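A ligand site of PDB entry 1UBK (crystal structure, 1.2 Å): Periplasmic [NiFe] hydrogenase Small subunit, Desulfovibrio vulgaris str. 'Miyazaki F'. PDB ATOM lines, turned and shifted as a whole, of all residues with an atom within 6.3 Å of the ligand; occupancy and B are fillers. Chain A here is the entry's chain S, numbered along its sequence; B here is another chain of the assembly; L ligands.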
ATOM      1  N   ALA A  15     -25.282 -21.949  20.997  1.00  0.00           N
ATOM      2  CA  ALA A  15     -23.957 -21.929  21.658  1.00  0.00           C
ATOM      3  C   ALA A  15     -23.032 -21.188  20.715  1.00  0.00           C
ATOM      4  O   ALA A  15     -22.603 -21.748  19.715  1.00  0.00           O
ATOM      5  CB  ALA A  15     -23.488 -23.342  21.958  1.00  0.00           C
ATOM      6  N   GLU A  16     -22.771 -19.916  21.055  1.00  0.00           N
ATOM      7  CA  GLU A  16     -22.102 -19.048  20.075  1.00  0.00           C
ATOM      8  C   GLU A  16     -21.314 -18.004  20.847  1.00  0.00           C
ATOM      9  O   GLU A  16     -21.507 -17.830  22.053  1.00  0.00           O
ATOM     10  CB  GLU A  16     -23.134 -18.371  19.154  1.00  0.00           C
ATOM     11  CG  GLU A  16     -24.404 -17.829  19.835  1.00  0.00           C
ATOM     12  CD  GLU A  16     -24.297 -16.504  20.522  1.00  0.00           C
ATOM     13  OE1 GLU A  16     -23.630 -15.626  19.956  1.00  0.00           O
ATOM     14  OE2 GLU A  16     -24.921 -16.333  21.572  1.00  0.00           O
ATOM     15  N   CYS A  17     -20.415 -17.312  20.139  1.00  0.00           N
ATOM     16  CA  CYS A  17     -19.579 -16.312  20.721  1.00  0.00           C
ATOM     17  C   CYS A  17     -20.019 -14.907  20.302  1.00  0.00           C
ATOM     18  O   CYS A  17     -19.407 -13.945  20.755  1.00  0.00           O
ATOM     19  CB  CYS A  17     -18.110 -16.488  20.297  1.00  0.00           C
ATOM     20  SG  CYS A  17     -17.673 -15.957  18.624  1.00  0.00           S
ATOM     21  N   THR A  18     -21.007 -14.816  19.428  1.00  0.00           N
ATOM     22  CA  THR A  18     -21.592 -13.575  18.881  1.00  0.00           C
ATOM     23  C   THR A  18     -20.693 -12.938  17.833  1.00  0.00           C
ATOM     24  O   THR A  18     -21.032 -11.893  17.243  1.00  0.00           O
ATOM     25  CB  THR A  18     -21.999 -12.631  20.045  1.00  0.00           C
ATOM     26  OG1 THR A  18     -22.719 -13.414  21.028  1.00  0.00           O
ATOM     27  CG2 THR A  18     -22.886 -11.500  19.539  1.00  0.00           C
ATOM     28  N   GLY A  19     -19.586 -13.614  17.480  1.00  0.00           N
ATOM     29  CA  GLY A  19     -18.780 -13.142  16.363  1.00  0.00           C
ATOM     30  C   GLY A  19     -19.491 -13.201  15.057  1.00  0.00           C
ATOM     31  O   GLY A  19     -19.281 -12.383  14.166  1.00  0.00           O
ATOM     32  N   CYS A  20     -20.387 -14.205  14.862  1.00  0.00           N
ATOM     33  CA  CYS A  20     -21.170 -14.212  13.636  1.00  0.00           C
ATOM     34  C   CYS A  20     -22.129 -13.033  13.607  1.00  0.00           C
ATOM     35  O   CYS A  20     -22.233 -12.366  12.568  1.00  0.00           O
ATOM     36  CB  CYS A  20     -21.880 -15.557  13.516  1.00  0.00           C
ATOM     37  SG  CYS A  20     -20.748 -16.903  13.060  1.00  0.00           S
ATOM     38  N   SER A  21     -22.811 -12.735  14.711  1.00  0.00           N
ATOM     39  CA  SER A  21     -23.663 -11.512  14.719  1.00  0.00           C
ATOM     40  C   SER A  21     -22.858 -10.267  14.410  1.00  0.00           C
ATOM     41  O   SER A  21     -23.304  -9.420  13.641  1.00  0.00           O
ATOM     42  CB  SER A  21     -24.303 -11.274  16.071  1.00  0.00           C
ATOM     43  OG  SER A  21     -25.329 -12.201  16.336  1.00  0.00           O
ATOM     44  N   GLU A  75     -27.261 -18.783  14.564  1.00  0.00           N
ATOM     45  CA  GLU A  75     -25.865 -18.690  14.971  1.00  0.00           C
ATOM     46  C   GLU A  75     -25.658 -19.605  16.165  1.00  0.00           C
ATOM     47  O   GLU A  75     -26.432 -19.612  17.118  1.00  0.00           O
ATOM     48  CB  GLU A  75     -25.557 -17.227  15.346  1.00  0.00           C
ATOM     49  CG  GLU A  75     -24.184 -16.958  15.988  1.00  0.00           C
ATOM     50  CD  GLU A  75     -23.963 -15.436  16.151  1.00  0.00           C
ATOM     51  OE1 GLU A  75     -22.827 -15.105  16.557  1.00  0.00           O
ATOM     52  OE2 GLU A  75     -24.913 -14.647  15.890  1.00  0.00           O
ATOM     53  N   GLY A  76     -24.577 -20.389  16.102  1.00  0.00           N
ATOM     54  CA  GLY A  76     -24.207 -21.225  17.230  1.00  0.00           C
ATOM     55  C   GLY A  76     -24.624 -22.693  17.036  1.00  0.00           C
ATOM     56  O   GLY A  76     -25.599 -23.039  16.367  1.00  0.00           O
ATOM     57  N   GLY A  77     -23.824 -23.567  17.667  1.00  0.00           N
ATOM     58  CA  GLY A  77     -24.158 -24.984  17.723  1.00  0.00           C
ATOM     59  C   GLY A  77     -25.250 -25.237  18.746  1.00  0.00           C
ATOM     60  O   GLY A  77     -25.496 -24.453  19.640  1.00  0.00           O
ATOM     61  N   TYR A 111     -25.606 -19.945   9.999  1.00  0.00           N
ATOM     62  CA  TYR A 111     -24.600 -18.902   9.746  1.00  0.00           C
ATOM     63  C   TYR A 111     -23.470 -19.097  10.737  1.00  0.00           C
ATOM     64  O   TYR A 111     -23.665 -18.953  11.950  1.00  0.00           O
ATOM     65  CB  TYR A 111     -25.255 -17.510   9.868  1.00  0.00           C
ATOM     66  CG  TYR A 111     -24.255 -16.410   9.456  1.00  0.00           C
ATOM     67  CD1 TYR A 111     -23.713 -16.392   8.175  1.00  0.00           C
ATOM     68  CD2 TYR A 111     -23.915 -15.425  10.371  1.00  0.00           C
ATOM     69  CE1 TYR A 111     -22.805 -15.399   7.763  1.00  0.00           C
ATOM     70  CE2 TYR A 111     -22.979 -14.450   9.977  1.00  0.00           C
ATOM     71  CZ  TYR A 111     -22.432 -14.437   8.719  1.00  0.00           C
ATOM     72  OH  TYR A 111     -21.535 -13.506   8.309  1.00  0.00           O
ATOM     73  N   GLY A 112     -22.289 -19.430  10.193  1.00  0.00           N
ATOM     74  CA  GLY A 112     -21.079 -19.694  10.984  1.00  0.00           C
ATOM     75  C   GLY A 112     -20.866 -21.193  11.162  1.00  0.00           C
ATOM     76  O   GLY A 112     -21.794 -21.985  11.265  1.00  0.00           O
ATOM     77  N   THR A 113     -19.551 -21.521  11.268  1.00  0.00           N
ATOM     78  CA  THR A 113     -19.168 -22.936  11.400  1.00  0.00           C
ATOM     79  C   THR A 113     -19.770 -23.580  12.618  1.00  0.00           C
ATOM     80  O   THR A 113     -20.026 -24.785  12.585  1.00  0.00           O
ATOM     81  CB  THR A 113     -17.630 -22.989  11.457  1.00  0.00           C
ATOM     82  OG1 THR A 113     -17.236 -22.596  10.120  1.00  0.00           O
ATOM     83  CG2 THR A 113     -17.065 -24.377  11.796  1.00  0.00           C
ATOM     84  N   CYS A 114     -20.079 -22.861  13.714  1.00  0.00           N
ATOM     85  CA  CYS A 114     -20.763 -23.519  14.808  1.00  0.00           C
ATOM     86  C   CYS A 114     -22.197 -23.956  14.413  1.00  0.00           C
ATOM     87  O   CYS A 114     -22.556 -25.103  14.663  1.00  0.00           O
ATOM     88  CB  CYS A 114     -20.955 -22.586  16.018  1.00  0.00           C
ATOM     89  SG  CYS A 114     -19.354 -22.077  16.774  1.00  0.00           S
ATOM     90  N   ALA A 115     -22.967 -23.073  13.784  1.00  0.00           N
ATOM     91  CA  ALA A 115     -24.297 -23.508  13.373  1.00  0.00           C
ATOM     92  C   ALA A 115     -24.234 -24.507  12.211  1.00  0.00           C
ATOM     93  O   ALA A 115     -25.080 -25.414  12.094  1.00  0.00           O
ATOM     94  CB  ALA A 115     -25.099 -22.277  12.920  1.00  0.00           C
ATOM     95  N   GLY A 119     -18.779 -26.498  15.362  1.00  0.00           N
ATOM     96  CA  GLY A 119     -17.865 -25.437  15.775  1.00  0.00           C
ATOM     97  C   GLY A 119     -17.082 -25.666  17.044  1.00  0.00           C
ATOM     98  O   GLY A 119     -16.809 -26.808  17.460  1.00  0.00           O
ATOM     99  N   VAL A 120     -16.675 -24.585  17.667  1.00  0.00           N
ATOM    100  CA  VAL A 120     -15.606 -24.641  18.669  1.00  0.00           C
ATOM    101  C   VAL A 120     -16.061 -25.499  19.834  1.00  0.00           C
ATOM    102  O   VAL A 120     -15.243 -26.274  20.362  1.00  0.00           O
ATOM    103  CB  VAL A 120     -15.167 -23.226  19.045  1.00  0.00           C
ATOM    104  CG1 VAL A 120     -16.236 -22.447  19.826  1.00  0.00           C
ATOM    105  CG2 VAL A 120     -13.852 -23.280  19.835  1.00  0.00           C
ATOM    106  N   GLN A 121     -17.290 -25.379  20.337  1.00  0.00           N
ATOM    107  CA  GLN A 121     -17.729 -26.173  21.469  1.00  0.00           C
ATOM    108  C   GLN A 121     -17.934 -27.634  21.077  1.00  0.00           C
ATOM    109  O   GLN A 121     -18.008 -28.471  22.004  1.00  0.00           O
ATOM    110  CB  GLN A 121     -19.012 -25.612  22.102  1.00  0.00           C
ATOM    111  CG  GLN A 121     -20.197 -25.458  21.142  1.00  0.00           C
ATOM    112  CD  GLN A 121     -20.145 -24.147  20.404  1.00  0.00           C
ATOM    113  OE1 GLN A 121     -19.873 -23.101  20.974  1.00  0.00           O
ATOM    114  NE2 GLN A 121     -20.370 -24.168  19.100  1.00  0.00           N
ATOM    115  N   GLY A 149     -17.588 -20.546   8.137  1.00  0.00           N
ATOM    116  CA  GLY A 149     -16.520 -19.637   8.452  1.00  0.00           C
ATOM    117  C   GLY A 149     -16.680 -19.262   9.929  1.00  0.00           C
ATOM    118  O   GLY A 149     -17.773 -19.377  10.506  1.00  0.00           O
ATOM    119  N   CYS A 150     -15.589 -18.745  10.514  1.00  0.00           N
ATOM    120  CA  CYS A 150     -15.593 -18.468  11.953  1.00  0.00           C
ATOM    121  C   CYS A 150     -15.038 -17.097  12.293  1.00  0.00           C
ATOM    122  O   CYS A 150     -13.925 -16.939  12.839  1.00  0.00           O
ATOM    123  CB  CYS A 150     -14.776 -19.605  12.646  1.00  0.00           C
ATOM    124  SG  CYS A 150     -14.964 -19.720  14.448  1.00  0.00           S
ATOM    125  N   PRO A 151     -15.793 -16.032  11.978  1.00  0.00           N
ATOM    126  CA  PRO A 151     -17.113 -16.077  11.344  1.00  0.00           C
ATOM    127  C   PRO A 151     -17.001 -16.038   9.828  1.00  0.00           C
ATOM    128  O   PRO A 151     -15.923 -15.783   9.227  1.00  0.00           O
ATOM    129  CB  PRO A 151     -17.745 -14.779  11.834  1.00  0.00           C
ATOM    130  CG  PRO A 151     -16.538 -13.817  11.909  1.00  0.00           C
ATOM    131  CD  PRO A 151     -15.407 -14.689  12.434  1.00  0.00           C
ATOM    132  N   PRO A 152     -18.103 -16.300   9.142  1.00  0.00           N
ATOM    133  CA  PRO A 152     -18.110 -16.213   7.680  1.00  0.00           C
ATOM    134  C   PRO A 152     -17.908 -14.784   7.228  1.00  0.00           C
ATOM    135  O   PRO A 152     -18.060 -13.809   7.988  1.00  0.00           O
ATOM    136  CB  PRO A 152     -19.545 -16.679   7.291  1.00  0.00           C
ATOM    137  CG  PRO A 152     -20.030 -17.406   8.535  1.00  0.00           C
ATOM    138  CD  PRO A 152     -19.441 -16.641   9.713  1.00  0.00           C
ATOM    139  N   TRP A 258     -11.429 -27.514  14.117  1.00  0.00           N
ATOM    140  CA  TRP A 258     -10.710 -27.456  15.372  1.00  0.00           C
ATOM    141  C   TRP A 258      -9.870 -28.710  15.640  1.00  0.00           C
ATOM    142  O   TRP A 258      -8.810 -28.626  16.257  1.00  0.00           O
ATOM    143  CB  TRP A 258     -11.697 -27.219  16.549  1.00  0.00           C
ATOM    144  CG  TRP A 258     -12.446 -25.925  16.348  1.00  0.00           C
ATOM    145  CD1 TRP A 258     -13.731 -25.734  15.904  1.00  0.00           C
ATOM    146  CD2 TRP A 258     -11.912 -24.612  16.563  1.00  0.00           C
ATOM    147  NE1 TRP A 258     -14.004 -24.381  15.844  1.00  0.00           N
ATOM    148  CE2 TRP A 258     -12.901 -23.670  16.241  1.00  0.00           C
ATOM    149  CE3 TRP A 258     -10.663 -24.141  16.975  1.00  0.00           C
ATOM    150  CZ2 TRP A 258     -12.702 -22.275  16.336  1.00  0.00           C
ATOM    151  CZ3 TRP A 258     -10.466 -22.785  17.079  1.00  0.00           C
ATOM    152  CH2 TRP A 258     -11.454 -21.865  16.751  1.00  0.00           C
ATOM    153  N   ARG B  41     -20.045 -23.740  27.366  1.00  0.00           N
ATOM    154  CA  ARG B  41     -19.367 -24.349  26.249  1.00  0.00           C
ATOM    155  C   ARG B  41     -18.209 -25.226  26.664  1.00  0.00           C
ATOM    156  O   ARG B  41     -17.993 -26.301  26.072  1.00  0.00           O
ATOM    157  CB  ARG B  41     -18.902 -23.293  25.238  1.00  0.00           C
ATOM    158  CG  ARG B  41     -20.057 -22.671  24.455  1.00  0.00           C
ATOM    159  CD  ARG B  41     -19.729 -21.502  23.553  1.00  0.00           C
ATOM    160  NE  ARG B  41     -19.183 -20.433  24.386  1.00  0.00           N
ATOM    161  CZ  ARG B  41     -18.273 -19.559  23.950  1.00  0.00           C
ATOM    162  NH1 ARG B  41     -17.876 -19.445  22.698  1.00  0.00           N
ATOM    163  NH2 ARG B  41     -17.804 -18.701  24.871  1.00  0.00           N
ATOM    164  N   ARG B  61     -12.385 -17.482  20.275  1.00  0.00           N
ATOM    165  CA  ARG B  61     -13.800 -17.809  20.106  1.00  0.00           C
ATOM    166  C   ARG B  61     -14.533 -17.909  21.439  1.00  0.00           C
ATOM    167  O   ARG B  61     -15.712 -18.240  21.441  1.00  0.00           O
ATOM    168  CB  ARG B  61     -13.967 -19.090  19.285  1.00  0.00           C
ATOM    169  CG  ARG B  61     -13.805 -18.894  17.793  1.00  0.00           C
ATOM    170  CD  ARG B  61     -12.423 -18.444  17.400  1.00  0.00           C
ATOM    171  NE  ARG B  61     -12.379 -18.338  15.941  1.00  0.00           N
ATOM    172  CZ  ARG B  61     -11.315 -17.972  15.240  1.00  0.00           C
ATOM    173  NH1 ARG B  61     -10.155 -17.848  15.873  1.00  0.00           N
ATOM    174  NH2 ARG B  61     -11.446 -17.802  13.937  1.00  0.00           N
ATOM    175  N   GLY B  64     -16.825 -12.968  20.318  1.00  0.00           N
ATOM    176  CA  GLY B  64     -16.663 -12.163  19.081  1.00  0.00           C
ATOM    177  C   GLY B  64     -17.064 -10.720  19.261  1.00  0.00           C
ATOM    178  O   GLY B  64     -16.879  -9.986  18.260  1.00  0.00           O
ATOM    179  N   PRO B 216     -14.733  -9.724  12.551  1.00  0.00           N
ATOM    180  CA  PRO B 216     -14.234 -10.294  13.793  1.00  0.00           C
ATOM    181  C   PRO B 216     -13.170 -11.381  13.611  1.00  0.00           C
ATOM    182  O   PRO B 216     -13.008 -12.012  12.556  1.00  0.00           O
ATOM    183  CB  PRO B 216     -15.508 -10.948  14.446  1.00  0.00           C
ATOM    184  CG  PRO B 216     -16.668 -10.251  13.770  1.00  0.00           C
ATOM    185  CD  PRO B 216     -16.172 -10.027  12.342  1.00  0.00           C
ATOM    186  N   HIS B 217     -12.497 -11.584  14.743  1.00  0.00           N
ATOM    187  CA  HIS B 217     -11.513 -12.670  15.014  1.00  0.00           C
ATOM    188  C   HIS B 217     -10.269 -12.443  14.185  1.00  0.00           C
ATOM    189  O   HIS B 217     -10.057 -12.954  13.079  1.00  0.00           O
ATOM    190  CB  HIS B 217     -12.123 -14.065  14.827  1.00  0.00           C
ATOM    191  CG  HIS B 217     -13.128 -14.397  15.934  1.00  0.00           C
ATOM    192  ND1 HIS B 217     -14.086 -15.340  15.953  1.00  0.00           N
ATOM    193  CD2 HIS B 217     -13.168 -13.712  17.119  1.00  0.00           C
ATOM    194  CE1 HIS B 217     -14.725 -15.289  17.152  1.00  0.00           C
ATOM    195  NE2 HIS B 217     -14.157 -14.284  17.837  1.00  0.00           N
HETATM  196 FE1  LIG L   1     -18.213 -17.558  17.105  1.00  0.00          FE
HETATM  197 FE2  LIG L   1     -19.086 -19.912  16.237  1.00  0.00          FE
HETATM  198 FE3  LIG L   1     -16.955 -18.829  15.117  1.00  0.00          FE
HETATM  199 FE4  LIG L   1     -19.411 -17.686  14.684  1.00  0.00          FE
HETATM  200  S1  LIG L   1     -18.743 -19.726  13.955  1.00  0.00           S
HETATM  201  S2  LIG L   1     -17.421 -16.638  15.137  1.00  0.00           S
HETATM  202  S3  LIG L   1     -20.419 -18.140  16.720  1.00  0.00           S
HETATM  203  S4  LIG L   1     -17.135 -19.486  17.345  1.00  0.00           S
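O of Arg 61 of chain B sits at hydrogen-bond distance from NH1 of Arg 41 of chain B (2.8 Å). The side-chain carboxylate (OE1) of Glu 16 lies within hydrogen-bond range of the side-chain hydroxyl (OG1) of Thr 18, at 2.6 Å. The side-chain sulfur (SG) of Cys 20 sits close to the backbone carbonyl oxygen (O) of Tyr 111, at 3.7 Å. The side-chain amide nitrogen (NE2) of Gln 121 sits close to the side-chain sulfur (SG) of Cys 114, at 3.3 Å. NE of Arg 61 of chain B sits at hydrogen-bond distance from ND1 of His 217 of chain B (3.4 Å). The backbone carbonyl oxygen (O) of Cys 17 lies within hydrogen-bond range of the backbone NH (N) of Gly 64 of chain B, 2.8 Å away. The backbone carbonyl oxygen (O) of Cys 150 is in hydrogen-bond range of the guanidinium group (NH2) of Arg 61 of chain B, at 2.8 Å. The backbone NH (N) of Thr 18 sits close to the side-chain carboxylate (OE1) of Glu 75 (3.4 Å).
N of Cys 17 lies close to S3 of the ligand. SG of Cys 114 binds FE2 of the ligand (2.2 Å). An iron atom (FE4) of the ligand is bound by the side-chain sulfur (SG) of Cys 20, at 2.2 Å. An iron atom (FE1) of the ligand is bound by the side-chain sulfur (SG) of Cys 17. A ring nitrogen (ND1) of His 217 of chain B sits close to a sulfur (S2) of the ligand (3.7 Å). An iron atom (FE3) of the ligand is bound by the side-chain sulfur (SG) of Cys 150 (2.3 Å). N of Thr 113 lies close to S1 of the ligand (3.3 Å). S1 of the ligand lies close to N of Cys 114 (3.4 Å).
O of Gly 149 lies close to S1 of the ligand. The backbone nitrogen (N) of Pro 151 sits close to a sulfur (S2) of the ligand (3.6 Å). Merely in contact with the ligand: Arg 61 of chain B (3.4 Å), Glu 16 (3.7 Å), Gly 112 (3.8 Å), Glu 75 (3.9 Å), Gly 19 (3.9 Å) and Val 120 (3.97 Å). Hydrophobic or aromatic side chains that line the ligand: Val 120, Pro 151 and His 217 of chain B. Of the 28 residues printed, 14 come within 4 Å of the ligand. The nearest printed residue that does not touch the ligand is Thr 18 (4.3 Å).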
